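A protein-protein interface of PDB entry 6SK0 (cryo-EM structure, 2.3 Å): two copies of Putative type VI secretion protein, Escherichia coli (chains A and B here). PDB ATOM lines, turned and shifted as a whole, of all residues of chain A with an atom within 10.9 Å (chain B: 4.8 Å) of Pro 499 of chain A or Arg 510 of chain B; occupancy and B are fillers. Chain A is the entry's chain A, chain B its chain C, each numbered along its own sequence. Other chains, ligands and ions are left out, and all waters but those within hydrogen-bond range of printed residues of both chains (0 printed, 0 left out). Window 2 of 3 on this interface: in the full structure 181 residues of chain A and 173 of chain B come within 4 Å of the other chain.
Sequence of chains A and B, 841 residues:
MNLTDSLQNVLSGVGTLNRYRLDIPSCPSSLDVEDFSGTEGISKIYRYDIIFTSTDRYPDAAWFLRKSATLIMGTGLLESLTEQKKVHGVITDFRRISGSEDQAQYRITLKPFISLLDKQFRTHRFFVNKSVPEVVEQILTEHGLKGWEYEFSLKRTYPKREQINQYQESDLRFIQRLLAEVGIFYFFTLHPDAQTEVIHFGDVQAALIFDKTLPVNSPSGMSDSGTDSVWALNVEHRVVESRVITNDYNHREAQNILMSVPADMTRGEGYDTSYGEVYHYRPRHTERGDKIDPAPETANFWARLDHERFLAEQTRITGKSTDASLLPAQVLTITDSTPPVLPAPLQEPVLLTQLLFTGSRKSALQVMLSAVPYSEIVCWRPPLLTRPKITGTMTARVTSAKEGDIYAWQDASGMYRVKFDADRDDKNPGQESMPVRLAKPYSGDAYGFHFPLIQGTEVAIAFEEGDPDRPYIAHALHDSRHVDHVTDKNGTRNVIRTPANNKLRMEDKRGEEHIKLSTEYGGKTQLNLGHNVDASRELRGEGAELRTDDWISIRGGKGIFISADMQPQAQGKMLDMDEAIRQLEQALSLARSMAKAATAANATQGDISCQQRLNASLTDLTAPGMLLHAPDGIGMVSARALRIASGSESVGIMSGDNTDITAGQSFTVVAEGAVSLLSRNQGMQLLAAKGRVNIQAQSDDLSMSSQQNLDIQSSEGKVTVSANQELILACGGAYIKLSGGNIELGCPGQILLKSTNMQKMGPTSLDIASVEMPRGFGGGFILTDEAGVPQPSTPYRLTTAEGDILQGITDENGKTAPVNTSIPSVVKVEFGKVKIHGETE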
ATOM      1  N   VAL A 495      15.967   6.563  24.398  1.00  0.00           N
ATOM      2  CA  VAL A 495      15.611   7.922  24.778  1.00  0.00           C
ATOM      3  C   VAL A 495      14.488   8.409  23.880  1.00  0.00           C
ATOM      4  O   VAL A 495      14.627   8.416  22.651  1.00  0.00           O
ATOM      5  CB  VAL A 495      16.812   8.874  24.693  1.00  0.00           C
ATOM      6  CG1 VAL A 495      16.471  10.196  25.340  1.00  0.00           C
ATOM      7  CG2 VAL A 495      18.025   8.256  25.360  1.00  0.00           C
ATOM      8  N   ILE A 496      13.383   8.819  24.491  1.00  0.00           N
ATOM      9  CA  ILE A 496      12.349   9.604  23.836  1.00  0.00           C
ATOM     10  C   ILE A 496      12.576  11.048  24.263  1.00  0.00           C
ATOM     11  O   ILE A 496      12.095  11.478  25.312  1.00  0.00           O
ATOM     12  CB  ILE A 496      10.948   9.121  24.207  1.00  0.00           C
ATOM     13  CG1 ILE A 496      10.765   7.664  23.794  1.00  0.00           C
ATOM     14  CG2 ILE A 496       9.892  10.008  23.577  1.00  0.00           C
ATOM     15  CD1 ILE A 496       9.380   7.141  24.047  1.00  0.00           C
ATOM     16  N   ARG A 497      13.325  11.797  23.464  1.00  0.00           N
ATOM     17  CA  ARG A 497      13.700  13.162  23.795  1.00  0.00           C
ATOM     18  C   ARG A 497      13.018  14.126  22.838  1.00  0.00           C
ATOM     19  O   ARG A 497      13.064  13.935  21.620  1.00  0.00           O
ATOM     20  CB  ARG A 497      15.216  13.345  23.741  1.00  0.00           C
ATOM     21  CG  ARG A 497      15.719  14.523  24.542  1.00  0.00           C
ATOM     22  CD  ARG A 497      17.084  14.971  24.076  1.00  0.00           C
ATOM     23  NE  ARG A 497      17.006  15.829  22.897  1.00  0.00           N
ATOM     24  CZ  ARG A 497      16.906  17.154  22.938  1.00  0.00           C
ATOM     25  NH1 ARG A 497      16.871  17.784  24.103  1.00  0.00           N
ATOM     26  NH2 ARG A 497      16.840  17.849  21.813  1.00  0.00           N
ATOM     27  N   THR A 498      12.392  15.137  23.386  1.00  0.00           N
ATOM     28  CA  THR A 498      11.803  16.198  22.594  1.00  0.00           C
ATOM     29  C   THR A 498      12.797  17.339  22.440  1.00  0.00           C
ATOM     30  O   THR A 498      13.791  17.406  23.163  1.00  0.00           O
ATOM     31  CB  THR A 498      10.521  16.698  23.256  1.00  0.00           C
ATOM     32  OG1 THR A 498      10.848  17.540  24.370  1.00  0.00           O
ATOM     33  CG2 THR A 498       9.667  15.544  23.718  1.00  0.00           C
ATOM     34  N   PRO A 499      12.576  18.240  21.481  1.00  0.00           N
ATOM     35  CA  PRO A 499      13.493  19.383  21.340  1.00  0.00           C
ATOM     36  C   PRO A 499      13.582  20.252  22.581  1.00  0.00           C
ATOM     37  O   PRO A 499      14.624  20.877  22.812  1.00  0.00           O
ATOM     38  CB  PRO A 499      12.903  20.151  20.153  1.00  0.00           C
ATOM     39  CG  PRO A 499      12.206  19.119  19.364  1.00  0.00           C
ATOM     40  CD  PRO A 499      11.635  18.157  20.352  1.00  0.00           C
ATOM     41  N   ALA A 500      12.529  20.311  23.389  1.00  0.00           N
ATOM     42  CA  ALA A 500      12.558  21.062  24.634  1.00  0.00           C
ATOM     43  C   ALA A 500      13.210  20.295  25.771  1.00  0.00           C
ATOM     44  O   ALA A 500      13.175  20.764  26.910  1.00  0.00           O
ATOM     45  CB  ALA A 500      11.143  21.469  25.038  1.00  0.00           C
ATOM     46  N   ASN A 501      13.794  19.134  25.482  1.00  0.00           N
ATOM     47  CA  ASN A 501      14.446  18.268  26.456  1.00  0.00           C
ATOM     48  C   ASN A 501      13.472  17.661  27.460  1.00  0.00           C
ATOM     49  O   ASN A 501      13.867  17.318  28.573  1.00  0.00           O
ATOM     50  CB  ASN A 501      15.578  18.993  27.193  1.00  0.00           C
ATOM     51  CG  ASN A 501      16.695  18.060  27.600  1.00  0.00           C
ATOM     52  OD1 ASN A 501      17.018  17.116  26.885  1.00  0.00           O
ATOM     53  ND2 ASN A 501      17.287  18.313  28.760  1.00  0.00           N
ATOM     54  N   ASN A 502      12.201  17.523  27.100  1.00  0.00           N
ATOM     55  CA  ASN A 502      11.357  16.538  27.758  1.00  0.00           C
ATOM     56  C   ASN A 502      11.834  15.164  27.335  1.00  0.00           C
ATOM     57  O   ASN A 502      11.865  14.854  26.141  1.00  0.00           O
ATOM     58  CB  ASN A 502       9.891  16.715  27.384  1.00  0.00           C
ATOM     59  CG  ASN A 502       9.318  18.007  27.874  1.00  0.00           C
ATOM     60  OD1 ASN A 502       8.504  18.619  27.203  1.00  0.00           O
ATOM     61  ND2 ASN A 502       9.738  18.433  29.050  1.00  0.00           N
ATOM     62  N   LYS A 503      12.233  14.345  28.291  1.00  0.00           N
ATOM     63  CA  LYS A 503      12.802  13.060  27.936  1.00  0.00           C
ATOM     64  C   LYS A 503      12.179  11.958  28.769  1.00  0.00           C
ATOM     65  O   LYS A 503      11.821  12.149  29.932  1.00  0.00           O
ATOM     66  CB  LYS A 503      14.324  13.053  28.102  1.00  0.00           C
ATOM     67  CG  LYS A 503      14.796  13.434  29.474  1.00  0.00           C
ATOM     68  CD  LYS A 503      16.295  13.286  29.595  1.00  0.00           C
ATOM     69  CE  LYS A 503      17.013  14.090  28.534  1.00  0.00           C
ATOM     70  NZ  LYS A 503      18.483  13.914  28.636  1.00  0.00           N
ATOM     71  N   LEU A 504      12.028  10.808  28.134  1.00  0.00           N
ATOM     72  CA  LEU A 504      11.806   9.540  28.809  1.00  0.00           C
ATOM     73  C   LEU A 504      12.993   8.670  28.424  1.00  0.00           C
ATOM     74  O   LEU A 504      13.079   8.187  27.292  1.00  0.00           O
ATOM     75  CB  LEU A 504      10.479   8.913  28.415  1.00  0.00           C
ATOM     76  CG  LEU A 504      10.320   7.447  28.808  1.00  0.00           C
ATOM     77  CD1 LEU A 504      10.484   7.268  30.300  1.00  0.00           C
ATOM     78  CD2 LEU A 504       8.985   6.918  28.351  1.00  0.00           C
ATOM     79  N   SER A 518      11.874  13.281  32.663  1.00  0.00           N
ATOM     80  CA  SER A 518      12.411  14.564  33.081  1.00  0.00           C
ATOM     81  C   SER A 518      11.916  15.682  32.182  1.00  0.00           C
ATOM     82  O   SER A 518      11.920  15.552  30.956  1.00  0.00           O
ATOM     83  CB  SER A 518      13.942  14.532  33.087  1.00  0.00           C
ATOM     84  OG  SER A 518      14.477  15.820  33.294  1.00  0.00           O
ATOM     85  N   THR A 519      11.501  16.775  32.802  1.00  0.00           N
ATOM     86  CA  THR A 519      11.214  18.018  32.114  1.00  0.00           C
ATOM     87  C   THR A 519      12.145  19.098  32.642  1.00  0.00           C
ATOM     88  O   THR A 519      12.594  19.047  33.790  1.00  0.00           O
ATOM     89  CB  THR A 519       9.739  18.436  32.287  1.00  0.00           C
ATOM     90  OG1 THR A 519       9.495  19.643  31.566  1.00  0.00           O
ATOM     91  CG2 THR A 519       9.392  18.654  33.742  1.00  0.00           C
ATOM     92  N   GLU A 520      12.448  20.072  31.791  1.00  0.00           N
ATOM     93  CA  GLU A 520      13.319  21.169  32.184  1.00  0.00           C
ATOM     94  C   GLU A 520      12.623  22.202  33.051  1.00  0.00           C
ATOM     95  O   GLU A 520      13.297  23.067  33.610  1.00  0.00           O
ATOM     96  CB  GLU A 520      13.886  21.865  30.948  1.00  0.00           C
ATOM     97  CG  GLU A 520      14.987  21.100  30.269  1.00  0.00           C
ATOM     98  CD  GLU A 520      16.227  21.001  31.120  1.00  0.00           C
ATOM     99  OE1 GLU A 520      16.667  22.037  31.654  1.00  0.00           O
ATOM    100  OE2 GLU A 520      16.761  19.884  31.265  1.00  0.00           O
ATOM    101  N   TYR A 521      11.306  22.144  33.169  1.00  0.00           N
ATOM    102  CA  TYR A 521      10.587  23.142  33.936  1.00  0.00           C
ATOM    103  C   TYR A 521      10.766  22.904  35.431  1.00  0.00           C
ATOM    104  O   TYR A 521      10.836  21.763  35.889  1.00  0.00           O
ATOM    105  CB  TYR A 521       9.109  23.117  33.565  1.00  0.00           C
ATOM    106  CG  TYR A 521       8.340  24.265  34.139  1.00  0.00           C
ATOM    107  CD1 TYR A 521       7.786  24.187  35.404  1.00  0.00           C
ATOM    108  CD2 TYR A 521       8.176  25.436  33.423  1.00  0.00           C
ATOM    109  CE1 TYR A 521       7.096  25.231  35.936  1.00  0.00           C
ATOM    110  CE2 TYR A 521       7.486  26.491  33.950  1.00  0.00           C
ATOM    111  CZ  TYR A 521       6.947  26.384  35.206  1.00  0.00           C
ATOM    112  OH  TYR A 521       6.250  27.434  35.736  1.00  0.00           O
ATOM    113  N   GLY A 522      10.835  23.994  36.190  1.00  0.00           N
ATOM    114  CA  GLY A 522      10.986  23.932  37.629  1.00  0.00           C
ATOM    115  C   GLY A 522      12.299  23.316  38.050  1.00  0.00           C
ATOM    116  O   GLY A 522      12.322  22.354  38.821  1.00  0.00           O
ATOM    117  N   ASP B 508       6.204  20.835  24.782  1.00  0.00           N
ATOM    118  CA  ASP B 508       7.494  21.398  24.419  1.00  0.00           C
ATOM    119  C   ASP B 508       7.551  22.912  24.479  1.00  0.00           C
ATOM    120  O   ASP B 508       8.631  23.473  24.288  1.00  0.00           O
ATOM    121  CB  ASP B 508       7.880  20.963  23.011  1.00  0.00           C
ATOM    122  CG  ASP B 508       8.381  19.562  22.962  1.00  0.00           C
ATOM    123  OD1 ASP B 508       9.481  19.378  22.412  1.00  0.00           O
ATOM    124  OD2 ASP B 508       7.699  18.657  23.488  1.00  0.00           O
ATOM    125  N   LYS B 509       6.435  23.586  24.719  1.00  0.00           N
ATOM    126  CA  LYS B 509       6.439  25.041  24.679  1.00  0.00           C
ATOM    127  C   LYS B 509       7.461  25.583  25.665  1.00  0.00           C
ATOM    128  O   LYS B 509       7.384  25.310  26.867  1.00  0.00           O
ATOM    129  CB  LYS B 509       5.049  25.585  24.985  1.00  0.00           C
ATOM    130  CG  LYS B 509       4.977  27.090  24.944  1.00  0.00           C
ATOM    131  CD  LYS B 509       3.828  27.614  25.756  1.00  0.00           C
ATOM    132  CE  LYS B 509       3.180  28.784  25.058  1.00  0.00           C
ATOM    133  NZ  LYS B 509       2.085  29.349  25.875  1.00  0.00           N
ATOM    134  N   ARG B 510       8.438  26.318  25.142  1.00  0.00           N
ATOM    135  CA  ARG B 510       9.580  26.743  25.937  1.00  0.00           C
ATOM    136  C   ARG B 510       9.134  27.586  27.120  1.00  0.00           C
ATOM    137  O   ARG B 510       8.261  28.446  26.996  1.00  0.00           O
ATOM    138  CB  ARG B 510      10.563  27.526  25.073  1.00  0.00           C
ATOM    139  CG  ARG B 510      11.072  26.758  23.875  1.00  0.00           C
ATOM    140  CD  ARG B 510      11.511  25.361  24.256  1.00  0.00           C
ATOM    141  NE  ARG B 510      12.333  24.757  23.214  1.00  0.00           N
ATOM    142  CZ  ARG B 510      11.856  24.075  22.179  1.00  0.00           C
ATOM    143  NH1 ARG B 510      12.691  23.574  21.284  1.00  0.00           N
ATOM    144  NH2 ARG B 510      10.552  23.891  22.038  1.00  0.00           N
ATOM    145  N   GLY B 511       9.733  27.320  28.274  1.00  0.00           N
ATOM    146  CA  GLY B 511       9.341  27.974  29.495  1.00  0.00           C
ATOM    147  C   GLY B 511       8.067  27.458  30.115  1.00  0.00           C
ATOM    148  O   GLY B 511       7.735  27.871  31.228  1.00  0.00           O
ATOM    149  N   GLU B 512       7.327  26.593  29.425  1.00  0.00           N
ATOM    150  CA  GLU B 512       6.134  25.969  29.983  1.00  0.00           C
ATOM    151  C   GLU B 512       6.102  24.481  29.677  1.00  0.00           C
ATOM    152  O   GLU B 512       5.039  23.923  29.400  1.00  0.00           O
ATOM    153  CB  GLU B 512       4.862  26.634  29.465  1.00  0.00           C
ATOM    154  CG  GLU B 512       4.803  28.120  29.721  1.00  0.00           C
ATOM    155  CD  GLU B 512       3.525  28.746  29.228  1.00  0.00           C
ATOM    156  OE1 GLU B 512       3.357  29.968  29.412  1.00  0.00           O
ATOM    157  OE2 GLU B 512       2.685  28.022  28.661  1.00  0.00           O
ATOM    158  N   GLU B 513       7.253  23.831  29.723  1.00  0.00           N
ATOM    159  CA  GLU B 513       7.329  22.414  29.417  1.00  0.00           C
ATOM    160  C   GLU B 513       6.660  21.600  30.511  1.00  0.00           C
ATOM    161  O   GLU B 513       6.700  21.957  31.689  1.00  0.00           O
ATOM    162  CB  GLU B 513       8.784  21.985  29.261  1.00  0.00           C
ATOM    163  CG  GLU B 513       9.605  22.884  28.355  1.00  0.00           C
ATOM    164  CD  GLU B 513      10.202  24.077  29.084  1.00  0.00           C
ATOM    165  OE1 GLU B 513       9.773  24.367  30.216  1.00  0.00           O
ATOM    166  OE2 GLU B 513      11.098  24.728  28.522  1.00  0.00           O
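No position is printed for both chains.
Of the 11 pairs that touch across the chains among the printed residues, none has its exchanged pair printed and touching as well.
Arg 510 of chain B touches Pro 499 of chain A.
Arg 510 of chain B touches Ala 500 of chain A.
Glu 513 of chain B touches Ala 500 of chain A.
Asn 502 of chain A touches Asp 508 of chain B.
ND2 of Asn 502 of chain A touches CB of Glu 513 of chain B, 3.7 Å away.
OG1 of Thr 519 of chain A touches CB of Glu 513 of chain B, 3.4 Å away.
O of Gly 511 of chain B touches CE2 of Tyr 521 of chain A, 3.1 Å away.
CB of Tyr 521 of chain A touches O of Glu 513 of chain B (3.3 Å).
Of the 15 printed residues of chain A, 6 touch a printed residue of chain B.
Among the printed residues, 11 pairs touch across the chains.
OG1 of Thr 498 of chain A sits close to N of Ala 500 of chain A (3.4 Å).
The backbone NH of Asn 502 of chain A sits at hydrogen-bond distance from the side-chain hydroxyl of Thr 498 of chain A (3.0 Å).
The side-chain amide nitrogen (ND2) of Asn 502 of chain A sits at hydrogen-bond distance from the side-chain hydroxyl (OG1) of Thr 519 of chain A (2.8 Å).
The side-chain hydroxyl (OG1) of Thr 519 of chain A sits close to the backbone NH (N) of Tyr 521 of chain A, 3.5 Å away.
The guanidinium group of Arg 510 of chain B sits at hydrogen-bond distance from the backbone carbonyl oxygen of Asp 508 of chain B (3.0 Å).
The backbone NH (N) of Gly 511 of chain B is in hydrogen-bond range of the side-chain carboxylate (OE2) of Glu 513 of chain B (2.9 Å).
Of chain B, only Asp 508 (3.2 Å) and Arg 510 (3.6 Å) come within 4 Å of Pro 499 of chain A.
Arg 510 of chain B touches two residues of chain A.
Lys 509 of chain B touches none of the printed residues of chain A.
Printed residues of chain A within 4 Å of Gly 511 of chain B: Tyr 521 (3.1 Å).
No residue of chain A comes within 4 Å of Glu 512 of chain B.
Of the printed residues of chain B, Thr 519 of chain A touches Glu 513 (3.4 Å).
Printed residues of chain B within 4 Å of Ala 500 of chain A: Asp 508 (3.3 Å), Arg 510 (3.9 Å) and Glu 513 (3.9 Å).
Of the printed residues of chain A, Glu 513 of chain B touches Ala 500, Asn 502, Thr 519 and Tyr 521.
The nearest printed residue of chain B that does not touch Pro 499 of chain A is Glu 513 of chain B (7.5 Å).
The nearest residue of chain A that does not touch Arg 510 of chain B is Asn 501 of chain A (6.2 Å).
The nearest printed residue of chain A that does not touch Glu 513 of chain B is Glu 520 of chain A (4.6 Å).
OD1 of Asp 508 of chain B sits close to OG1 of Thr 498 of chain A (3.0 Å).
The side-chain carboxylate (OD1) of Asp 508 of chain B is in hydrogen-bond range of the backbone NH (N) of Ala 500 of chain A (3.3 Å).
The side-chain carboxylate of Asp 508 of chain B lies close to the backbone nitrogen of Pro 499 of chain A, 3.4 Å away.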
